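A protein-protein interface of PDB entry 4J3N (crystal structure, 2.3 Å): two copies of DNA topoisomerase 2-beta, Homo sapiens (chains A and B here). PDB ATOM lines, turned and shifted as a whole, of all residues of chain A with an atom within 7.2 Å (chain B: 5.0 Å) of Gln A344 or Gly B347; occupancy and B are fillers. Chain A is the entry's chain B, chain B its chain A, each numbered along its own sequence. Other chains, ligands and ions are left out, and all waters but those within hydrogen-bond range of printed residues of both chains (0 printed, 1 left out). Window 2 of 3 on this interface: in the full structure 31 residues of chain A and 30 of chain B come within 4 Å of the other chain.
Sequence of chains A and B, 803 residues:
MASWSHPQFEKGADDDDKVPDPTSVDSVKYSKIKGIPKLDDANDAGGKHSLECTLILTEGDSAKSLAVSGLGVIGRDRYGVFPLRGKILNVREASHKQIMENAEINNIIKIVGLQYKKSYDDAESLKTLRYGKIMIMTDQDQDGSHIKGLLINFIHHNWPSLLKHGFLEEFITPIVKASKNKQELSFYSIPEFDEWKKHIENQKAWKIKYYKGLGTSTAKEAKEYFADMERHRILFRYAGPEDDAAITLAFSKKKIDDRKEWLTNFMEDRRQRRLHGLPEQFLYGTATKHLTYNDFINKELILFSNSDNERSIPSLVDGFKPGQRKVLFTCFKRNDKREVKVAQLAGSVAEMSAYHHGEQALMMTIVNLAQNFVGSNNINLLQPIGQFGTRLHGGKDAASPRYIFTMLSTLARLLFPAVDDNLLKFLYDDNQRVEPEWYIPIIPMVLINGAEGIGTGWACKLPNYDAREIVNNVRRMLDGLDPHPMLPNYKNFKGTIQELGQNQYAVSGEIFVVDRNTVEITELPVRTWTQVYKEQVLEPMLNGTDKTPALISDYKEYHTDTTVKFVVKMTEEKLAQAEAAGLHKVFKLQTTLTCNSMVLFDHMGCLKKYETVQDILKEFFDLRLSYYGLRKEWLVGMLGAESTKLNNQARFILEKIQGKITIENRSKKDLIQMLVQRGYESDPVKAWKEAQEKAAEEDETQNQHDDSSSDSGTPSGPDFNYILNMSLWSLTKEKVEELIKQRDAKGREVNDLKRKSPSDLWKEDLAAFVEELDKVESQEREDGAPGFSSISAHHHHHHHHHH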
ATOM      1  N   THR A 330      18.530  10.694  25.489  1.00  0.00           N
ATOM      2  CA  THR A 330      19.394  11.622  26.220  1.00  0.00           C
ATOM      3  C   THR A 330      18.580  12.631  27.020  1.00  0.00           C
ATOM      4  O   THR A 330      18.888  12.901  28.177  1.00  0.00           O
ATOM      5  CB  THR A 330      20.367  12.373  25.271  1.00  0.00           C
ATOM      6  OG1 THR A 330      21.164  11.424  24.546  1.00  0.00           O
ATOM      7  CG2 THR A 330      21.276  13.295  26.059  1.00  0.00           C
ATOM      8  N   ARG A 334      18.804  12.955  31.020  1.00  0.00           N
ATOM      9  CA  ARG A 334      19.144  14.247  31.608  1.00  0.00           C
ATOM     10  C   ARG A 334      18.013  14.810  32.456  1.00  0.00           C
ATOM     11  O   ARG A 334      18.254  15.425  33.496  1.00  0.00           O
ATOM     12  CB  ARG A 334      19.465  15.268  30.520  1.00  0.00           C
ATOM     13  CG  ARG A 334      20.775  15.052  29.773  1.00  0.00           C
ATOM     14  CD  ARG A 334      20.897  16.116  28.697  1.00  0.00           C
ATOM     15  NE  ARG A 334      20.720  17.437  29.285  1.00  0.00           N
ATOM     16  CZ  ARG A 334      21.718  18.270  29.557  1.00  0.00           C
ATOM     17  NH1 ARG A 334      22.962  17.935  29.250  1.00  0.00           N
ATOM     18  NH2 ARG A 334      21.468  19.446  30.111  1.00  0.00           N
ATOM     19  N   VAL A 340      17.857  24.326  27.862  1.00  0.00           N
ATOM     20  CA  VAL A 340      19.229  23.916  27.621  1.00  0.00           C
ATOM     21  C   VAL A 340      19.622  24.289  26.200  1.00  0.00           C
ATOM     22  O   VAL A 340      18.858  24.047  25.261  1.00  0.00           O
ATOM     23  CB  VAL A 340      19.364  22.395  27.791  1.00  0.00           C
ATOM     24  CG1 VAL A 340      20.724  21.915  27.328  1.00  0.00           C
ATOM     25  CG2 VAL A 340      19.104  22.000  29.244  1.00  0.00           C
ATOM     26  N   LYS A 341      20.803  24.866  26.037  1.00  0.00           N
ATOM     27  CA  LYS A 341      21.264  25.283  24.716  1.00  0.00           C
ATOM     28  C   LYS A 341      21.294  24.078  23.778  1.00  0.00           C
ATOM     29  O   LYS A 341      21.757  23.001  24.149  1.00  0.00           O
ATOM     30  CB  LYS A 341      22.661  25.909  24.822  1.00  0.00           C
ATOM     31  CG  LYS A 341      22.989  26.913  23.739  1.00  0.00           C
ATOM     32  CD  LYS A 341      22.514  28.293  24.140  1.00  0.00           C
ATOM     33  CE  LYS A 341      23.316  28.808  25.324  1.00  0.00           C
ATOM     34  NZ  LYS A 341      24.699  29.202  24.931  1.00  0.00           N
ATOM     35  N   VAL A 342      20.796  24.241  22.560  1.00  0.00           N
ATOM     36  CA  VAL A 342      20.786  23.096  21.658  1.00  0.00           C
ATOM     37  C   VAL A 342      22.180  22.464  21.480  1.00  0.00           C
ATOM     38  O   VAL A 342      22.331  21.242  21.515  1.00  0.00           O
ATOM     39  CB  VAL A 342      20.097  23.430  20.315  1.00  0.00           C
ATOM     40  CG1 VAL A 342      20.348  22.332  19.285  1.00  0.00           C
ATOM     41  CG2 VAL A 342      18.587  23.640  20.547  1.00  0.00           C
ATOM     42  N   ALA A 343      23.203  23.291  21.311  1.00  0.00           N
ATOM     43  CA  ALA A 343      24.567  22.786  21.122  1.00  0.00           C
ATOM     44  C   ALA A 343      25.057  21.949  22.305  1.00  0.00           C
ATOM     45  O   ALA A 343      25.744  20.946  22.116  1.00  0.00           O
ATOM     46  CB  ALA A 343      25.527  23.941  20.851  1.00  0.00           C
ATOM     47  N   GLN A 344      24.708  22.348  23.527  1.00  0.00           N
ATOM     48  CA  GLN A 344      25.129  21.565  24.678  1.00  0.00           C
ATOM     49  C   GLN A 344      24.318  20.274  24.786  1.00  0.00           C
ATOM     50  O   GLN A 344      24.853  19.236  25.193  1.00  0.00           O
ATOM     51  CB  GLN A 344      25.060  22.381  25.976  1.00  0.00           C
ATOM     52  CG  GLN A 344      25.700  21.679  27.192  1.00  0.00           C
ATOM     53  CD  GLN A 344      27.231  21.810  27.249  1.00  0.00           C
ATOM     54  OE1 GLN A 344      27.886  22.143  26.255  1.00  0.00           O
ATOM     55  NE2 GLN A 344      27.797  21.551  28.426  1.00  0.00           N
ATOM     56  N   LEU A 345      23.040  20.318  24.405  1.00  0.00           N
ATOM     57  CA  LEU A 345      22.238  19.093  24.384  1.00  0.00           C
ATOM     58  C   LEU A 345      22.912  18.126  23.425  1.00  0.00           C
ATOM     59  O   LEU A 345      23.095  16.960  23.741  1.00  0.00           O
ATOM     60  CB  LEU A 345      20.784  19.355  23.959  1.00  0.00           C
ATOM     61  CG  LEU A 345      19.921  18.084  23.843  1.00  0.00           C
ATOM     62  CD1 LEU A 345      19.910  17.339  25.154  1.00  0.00           C
ATOM     63  CD2 LEU A 345      18.483  18.380  23.401  1.00  0.00           C
ATOM     64  N   ALA A 346      23.306  18.638  22.263  1.00  0.00           N
ATOM     65  CA  ALA A 346      23.902  17.812  21.224  1.00  0.00           C
ATOM     66  C   ALA A 346      25.167  17.150  21.747  1.00  0.00           C
ATOM     67  O   ALA A 346      25.372  15.941  21.589  1.00  0.00           O
ATOM     68  CB  ALA A 346      24.220  18.667  20.000  1.00  0.00           C
ATOM     69  N   GLY A 347      26.013  17.955  22.385  1.00  0.00           N
ATOM     70  CA  GLY A 347      27.227  17.444  22.986  1.00  0.00           C
ATOM     71  C   GLY A 347      26.876  16.357  23.974  1.00  0.00           C
ATOM     72  O   GLY A 347      27.506  15.299  24.023  1.00  0.00           O
ATOM     73  N   SER A 348      25.843  16.616  24.757  1.00  0.00           N
ATOM     74  CA  SER A 348      25.382  15.647  25.745  1.00  0.00           C
ATOM     75  C   SER A 348      24.876  14.375  25.050  1.00  0.00           C
ATOM     76  O   SER A 348      25.138  13.261  25.512  1.00  0.00           O
ATOM     77  CB  SER A 348      24.300  16.276  26.629  1.00  0.00           C
ATOM     78  OG  SER A 348      23.957  15.433  27.693  1.00  0.00           O
ATOM     79  N   VAL A 349      24.169  14.539  23.929  1.00  0.00           N
ATOM     80  CA  VAL A 349      23.699  13.384  23.161  1.00  0.00           C
ATOM     81  C   VAL A 349      24.871  12.534  22.680  1.00  0.00           C
ATOM     82  O   VAL A 349      24.846  11.317  22.792  1.00  0.00           O
ATOM     83  CB  VAL A 349      22.862  13.790  21.911  1.00  0.00           C
ATOM     84  CG1 VAL A 349      22.559  12.547  21.054  1.00  0.00           C
ATOM     85  CG2 VAL A 349      21.572  14.514  22.323  1.00  0.00           C
ATOM     86  N   ALA A 350      25.891  13.179  22.117  1.00  0.00           N
ATOM     87  CA  ALA A 350      27.052  12.442  21.609  1.00  0.00           C
ATOM     88  C   ALA A 350      27.712  11.636  22.724  1.00  0.00           C
ATOM     89  O   ALA A 350      28.082  10.481  22.546  1.00  0.00           O
ATOM     90  CB  ALA A 350      28.060  13.402  20.980  1.00  0.00           C
ATOM     91  N   GLU A 359      28.331  17.027  14.235  1.00  0.00           N
ATOM     92  CA  GLU A 359      27.352  17.721  15.047  1.00  0.00           C
ATOM     93  C   GLU A 359      26.367  18.609  14.257  1.00  0.00           C
ATOM     94  O   GLU A 359      25.261  18.871  14.740  1.00  0.00           O
ATOM     95  CB  GLU A 359      28.006  18.411  16.258  1.00  0.00           C
ATOM     96  CG  GLU A 359      28.327  17.419  17.420  1.00  0.00           C
ATOM     97  CD  GLU A 359      28.945  18.088  18.652  1.00  0.00           C
ATOM     98  OE1 GLU A 359      29.686  19.087  18.494  1.00  0.00           O
ATOM     99  OE2 GLU A 359      28.692  17.609  19.782  1.00  0.00           O
ATOM    100  N   MET A 363      22.431  18.655  15.426  1.00  0.00           N
ATOM    101  CA  MET A 363      21.760  19.895  15.776  1.00  0.00           C
ATOM    102  C   MET A 363      20.555  20.162  14.877  1.00  0.00           C
ATOM    103  O   MET A 363      19.525  20.643  15.342  1.00  0.00           O
ATOM    104  CB  MET A 363      22.765  21.055  15.789  1.00  0.00           C
ATOM    105  CG  MET A 363      23.622  21.009  17.086  1.00  0.00           C
ATOM    106  SD  MET A 363      25.034  22.102  17.045  1.00  0.00           S
ATOM    107  CE  MET A 363      26.108  21.318  18.249  1.00  0.00           C
ATOM    108  N   ILE A 366      17.829  17.900  16.130  1.00  0.00           N
ATOM    109  CA  ILE A 366      17.225  18.487  17.324  1.00  0.00           C
ATOM    110  C   ILE A 366      16.286  19.642  16.970  1.00  0.00           C
ATOM    111  O   ILE A 366      15.165  19.713  17.457  1.00  0.00           O
ATOM    112  CB  ILE A 366      18.297  18.941  18.365  1.00  0.00           C
ATOM    113  CG1 ILE A 366      18.996  17.725  18.974  1.00  0.00           C
ATOM    114  CG2 ILE A 366      17.660  19.750  19.496  1.00  0.00           C
ATOM    115  CD1 ILE A 366      20.375  18.018  19.542  1.00  0.00           C
ATOM    116  N   PRO A 401      22.308  27.010  16.409  1.00  0.00           N
ATOM    117  CA  PRO A 401      22.142  26.154  17.584  1.00  0.00           C
ATOM    118  C   PRO A 401      22.843  26.619  18.856  1.00  0.00           C
ATOM    119  O   PRO A 401      22.595  26.045  19.928  1.00  0.00           O
ATOM    120  CB  PRO A 401      22.669  24.787  17.117  1.00  0.00           C
ATOM    121  CG  PRO A 401      23.222  24.993  15.756  1.00  0.00           C
ATOM    122  CD  PRO A 401      22.610  26.229  15.201  1.00  0.00           C
ATOM    123  N   ARG A 402      23.694  27.633  18.761  1.00  0.00           N
ATOM    124  CA  ARG A 402      24.384  28.212  19.911  1.00  0.00           C
ATOM    125  C   ARG A 402      23.515  29.251  20.600  1.00  0.00           C
ATOM    126  O   ARG A 402      23.791  29.672  21.712  1.00  0.00           O
ATOM    127  CB  ARG A 402      25.672  28.909  19.456  1.00  0.00           C
ATOM    128  CG  ARG A 402      26.752  28.005  18.877  1.00  0.00           C
ATOM    129  CD  ARG A 402      28.010  28.825  18.549  1.00  0.00           C
ATOM    130  NE  ARG A 402      27.912  29.488  17.252  1.00  0.00           N
ATOM    131  CZ  ARG A 402      28.599  29.112  16.179  1.00  0.00           C
ATOM    132  NH1 ARG A 402      29.449  28.096  16.255  1.00  0.00           N
ATOM    133  NH2 ARG A 402      28.446  29.760  15.035  1.00  0.00           N
ATOM    134  N   ILE A 404      19.926  29.090  20.634  1.00  0.00           N
ATOM    135  CA  ILE A 404      18.575  28.611  20.904  1.00  0.00           C
ATOM    136  C   ILE A 404      18.565  27.523  21.959  1.00  0.00           C
ATOM    137  O   ILE A 404      19.564  26.837  22.186  1.00  0.00           O
ATOM    138  CB  ILE A 404      17.873  28.112  19.636  1.00  0.00           C
ATOM    139  CG1 ILE A 404      18.640  26.934  19.028  1.00  0.00           C
ATOM    140  CG2 ILE A 404      17.735  29.236  18.650  1.00  0.00           C
ATOM    141  CD1 ILE A 404      18.102  26.483  17.684  1.00  0.00           C
ATOM    142  N   ALA B 343      34.762  21.813  23.203  1.00  0.00           N
ATOM    143  CA  ALA B 343      33.524  22.502  22.864  1.00  0.00           C
ATOM    144  C   ALA B 343      32.458  22.289  23.949  1.00  0.00           C
ATOM    145  O   ALA B 343      31.709  23.212  24.293  1.00  0.00           O
ATOM    146  CB  ALA B 343      33.023  22.060  21.492  1.00  0.00           C
ATOM    147  N   GLN B 344      32.406  21.089  24.519  1.00  0.00           N
ATOM    148  CA  GLN B 344      31.414  20.812  25.547  1.00  0.00           C
ATOM    149  C   GLN B 344      31.805  21.439  26.885  1.00  0.00           C
ATOM    150  O   GLN B 344      30.944  21.955  27.618  1.00  0.00           O
ATOM    151  CB  GLN B 344      31.180  19.306  25.691  1.00  0.00           C
ATOM    152  CG  GLN B 344      29.981  18.946  26.556  1.00  0.00           C
ATOM    153  CD  GLN B 344      28.645  19.168  25.854  1.00  0.00           C
ATOM    154  OE1 GLN B 344      28.589  19.731  24.760  1.00  0.00           O
ATOM    155  NE2 GLN B 344      27.561  18.725  26.490  1.00  0.00           N
ATOM    156  N   LEU B 345      33.095  21.399  27.211  1.00  0.00           N
ATOM    157  CA  LEU B 345      33.570  22.077  28.413  1.00  0.00           C
ATOM    158  C   LEU B 345      33.166  23.554  28.343  1.00  0.00           C
ATOM    159  O   LEU B 345      32.693  24.136  29.316  1.00  0.00           O
ATOM    160  CB  LEU B 345      35.093  21.948  28.540  1.00  0.00           C
ATOM    161  CG  LEU B 345      35.723  22.777  29.663  1.00  0.00           C
ATOM    162  CD1 LEU B 345      35.083  22.420  30.979  1.00  0.00           C
ATOM    163  CD2 LEU B 345      37.240  22.573  29.717  1.00  0.00           C
ATOM    164  N   ALA B 346      33.352  24.163  27.178  1.00  0.00           N
ATOM    165  CA  ALA B 346      32.993  25.572  27.015  1.00  0.00           C
ATOM    166  C   ALA B 346      31.517  25.832  27.314  1.00  0.00           C
ATOM    167  O   ALA B 346      31.170  26.822  27.969  1.00  0.00           O
ATOM    168  CB  ALA B 346      33.335  26.053  25.607  1.00  0.00           C
ATOM    169  N   GLY B 347      30.646  24.952  26.814  1.00  0.00           N
ATOM    170  CA  GLY B 347      29.216  25.117  27.018  1.00  0.00           C
ATOM    171  C   GLY B 347      28.941  25.041  28.497  1.00  0.00           C
ATOM    172  O   GLY B 347      28.170  25.817  29.064  1.00  0.00           O
ATOM    173  N   SER B 348      29.606  24.085  29.126  1.00  0.00           N
ATOM    174  CA  SER B 348      29.537  23.907  30.561  1.00  0.00           C
ATOM    175  C   SER B 348      29.993  25.179  31.318  1.00  0.00           C
ATOM    176  O   SER B 348      29.341  25.597  32.283  1.00  0.00           O
ATOM    177  CB  SER B 348      30.367  22.674  30.940  1.00  0.00           C
ATOM    178  OG  SER B 348      30.272  22.366  32.310  1.00  0.00           O
ATOM    179  N   VAL B 349      31.084  25.810  30.870  1.00  0.00           N
ATOM    180  CA  VAL B 349      31.576  27.016  31.534  1.00  0.00           C
ATOM    181  C   VAL B 349      30.589  28.170  31.419  1.00  0.00           C
ATOM    182  O   VAL B 349      30.371  28.919  32.374  1.00  0.00           O
ATOM    183  CB  VAL B 349      32.924  27.500  30.965  1.00  0.00           C
ATOM    184  CG1 VAL B 349      33.305  28.831  31.621  1.00  0.00           C
ATOM    185  CG2 VAL B 349      34.019  26.443  31.158  1.00  0.00           C
ATOM    186  N   ALA B 350      30.022  28.339  30.233  1.00  0.00           N
ATOM    187  CA  ALA B 350      28.970  29.330  30.038  1.00  0.00           C
ATOM    188  C   ALA B 350      27.832  29.114  31.025  1.00  0.00           C
ATOM    189  O   ALA B 350      27.386  30.050  31.676  1.00  0.00           O
ATOM    190  CB  ALA B 350      28.444  29.293  28.598  1.00  0.00           C
ATOM    191  N   GLU B 351      27.374  27.876  31.161  1.00  0.00           N
ATOM    192  CA  GLU B 351      26.258  27.590  32.075  1.00  0.00           C
ATOM    193  C   GLU B 351      26.598  27.719  33.573  1.00  0.00           C
ATOM    194  O   GLU B 351      25.889  28.393  34.322  1.00  0.00           O
ATOM    195  CB  GLU B 351      25.629  26.227  31.747  1.00  0.00           C
ATOM    196  CG  GLU B 351      25.786  25.147  32.813  1.00  0.00           C
ATOM    197  CD  GLU B 351      25.630  23.727  32.247  1.00  0.00           C
ATOM    198  OE1 GLU B 351      24.861  23.566  31.267  1.00  0.00           O
ATOM    199  OE2 GLU B 351      26.283  22.782  32.771  1.00  0.00           O
ATOM    200  N   GLU B 359      31.236  31.884  22.160  1.00  0.00           N
ATOM    201  CA  GLU B 359      31.927  30.710  22.652  1.00  0.00           C
ATOM    202  C   GLU B 359      33.247  30.477  21.914  1.00  0.00           C
ATOM    203  O   GLU B 359      34.073  29.700  22.370  1.00  0.00           O
ATOM    204  CB  GLU B 359      31.005  29.480  22.693  1.00  0.00           C
ATOM    205  CG  GLU B 359      30.002  29.515  23.868  1.00  0.00           C
ATOM    206  CD  GLU B 359      29.092  28.290  23.934  1.00  0.00           C
ATOM    207  OE1 GLU B 359      29.362  27.304  23.214  1.00  0.00           O
ATOM    208  OE2 GLU B 359      28.104  28.315  24.707  1.00  0.00           O
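OE1 of Gln A344 lies close to OE1 of Gln B344 (2.9 Å). NE2 of Gln B344 lies close to N of Ser A348, at 3.2 Å. NE2 of Gln A344 sits close to N of Ser B348 (3.2 Å). The side-chain carboxylate (OE2) of Glu B359 lies within salt-bridge range of the side-chain amino group (NZ) of Lys A341, at 3.5 Å.
The guanidinium group (NH1) of Arg A334 sits at hydrogen-bond distance from the side-chain hydroxyl (OG) of Ser A348, at 3.1 Å. NZ of Lys A341 lies close to O of Arg A402 (3.4 Å).
Among the printed residues, merely in contact across the chains: Gly A347 with Gln B344 (3.2 Å) and Gln A344 with Gly B347 (3.3 Å).
Of the printed residues of chain B, Gln A344 touches Gln B344 (2.9 Å), Gly B347 (3.3 Å) and Ser B348 (3.2 Å). Printed residues of chain A within 4 Å of Gln B344: Gln A344 (2.9 Å), Gly A347 (3.2 Å) and Ser A348 (3.2 Å). Ala B346 touches none of the printed residues of chain A. Printed residues of chain A within 4 Å of Gly B347: Gln A344 (3.3 Å). Printed residues of chain A within 4 Å of Glu B359: Lys A341 (3.5 Å). The nearest printed residue of chain B that does not touch Gln A344 is Ala B343 (4.4 Å). The nearest printed residue of chain A that does not touch Gly B347 is Lys A341 (6.4 Å).
Of the 10 printed residues of chain B, 4 touch a printed residue of chain A. Printed residues of chain B that touch a printed residue of chain A: Gln B344, Gly B347, Ser B348 and Glu B359. Among the printed residues, Asp or Glu carboxylates within 4 Å of a Lys or Arg side-chain nitrogen of the other chain: Lys A341 with Glu B359 (3.5 Å).
Gln A344 touches its own counterpart, Gln B344. Gln A344 touches Gly B347, and with the chains exchanged Gly A347 touches Gln B344. Gln A344 touches Ser B348, and with the chains exchanged Ser A348 touches Gln B344.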
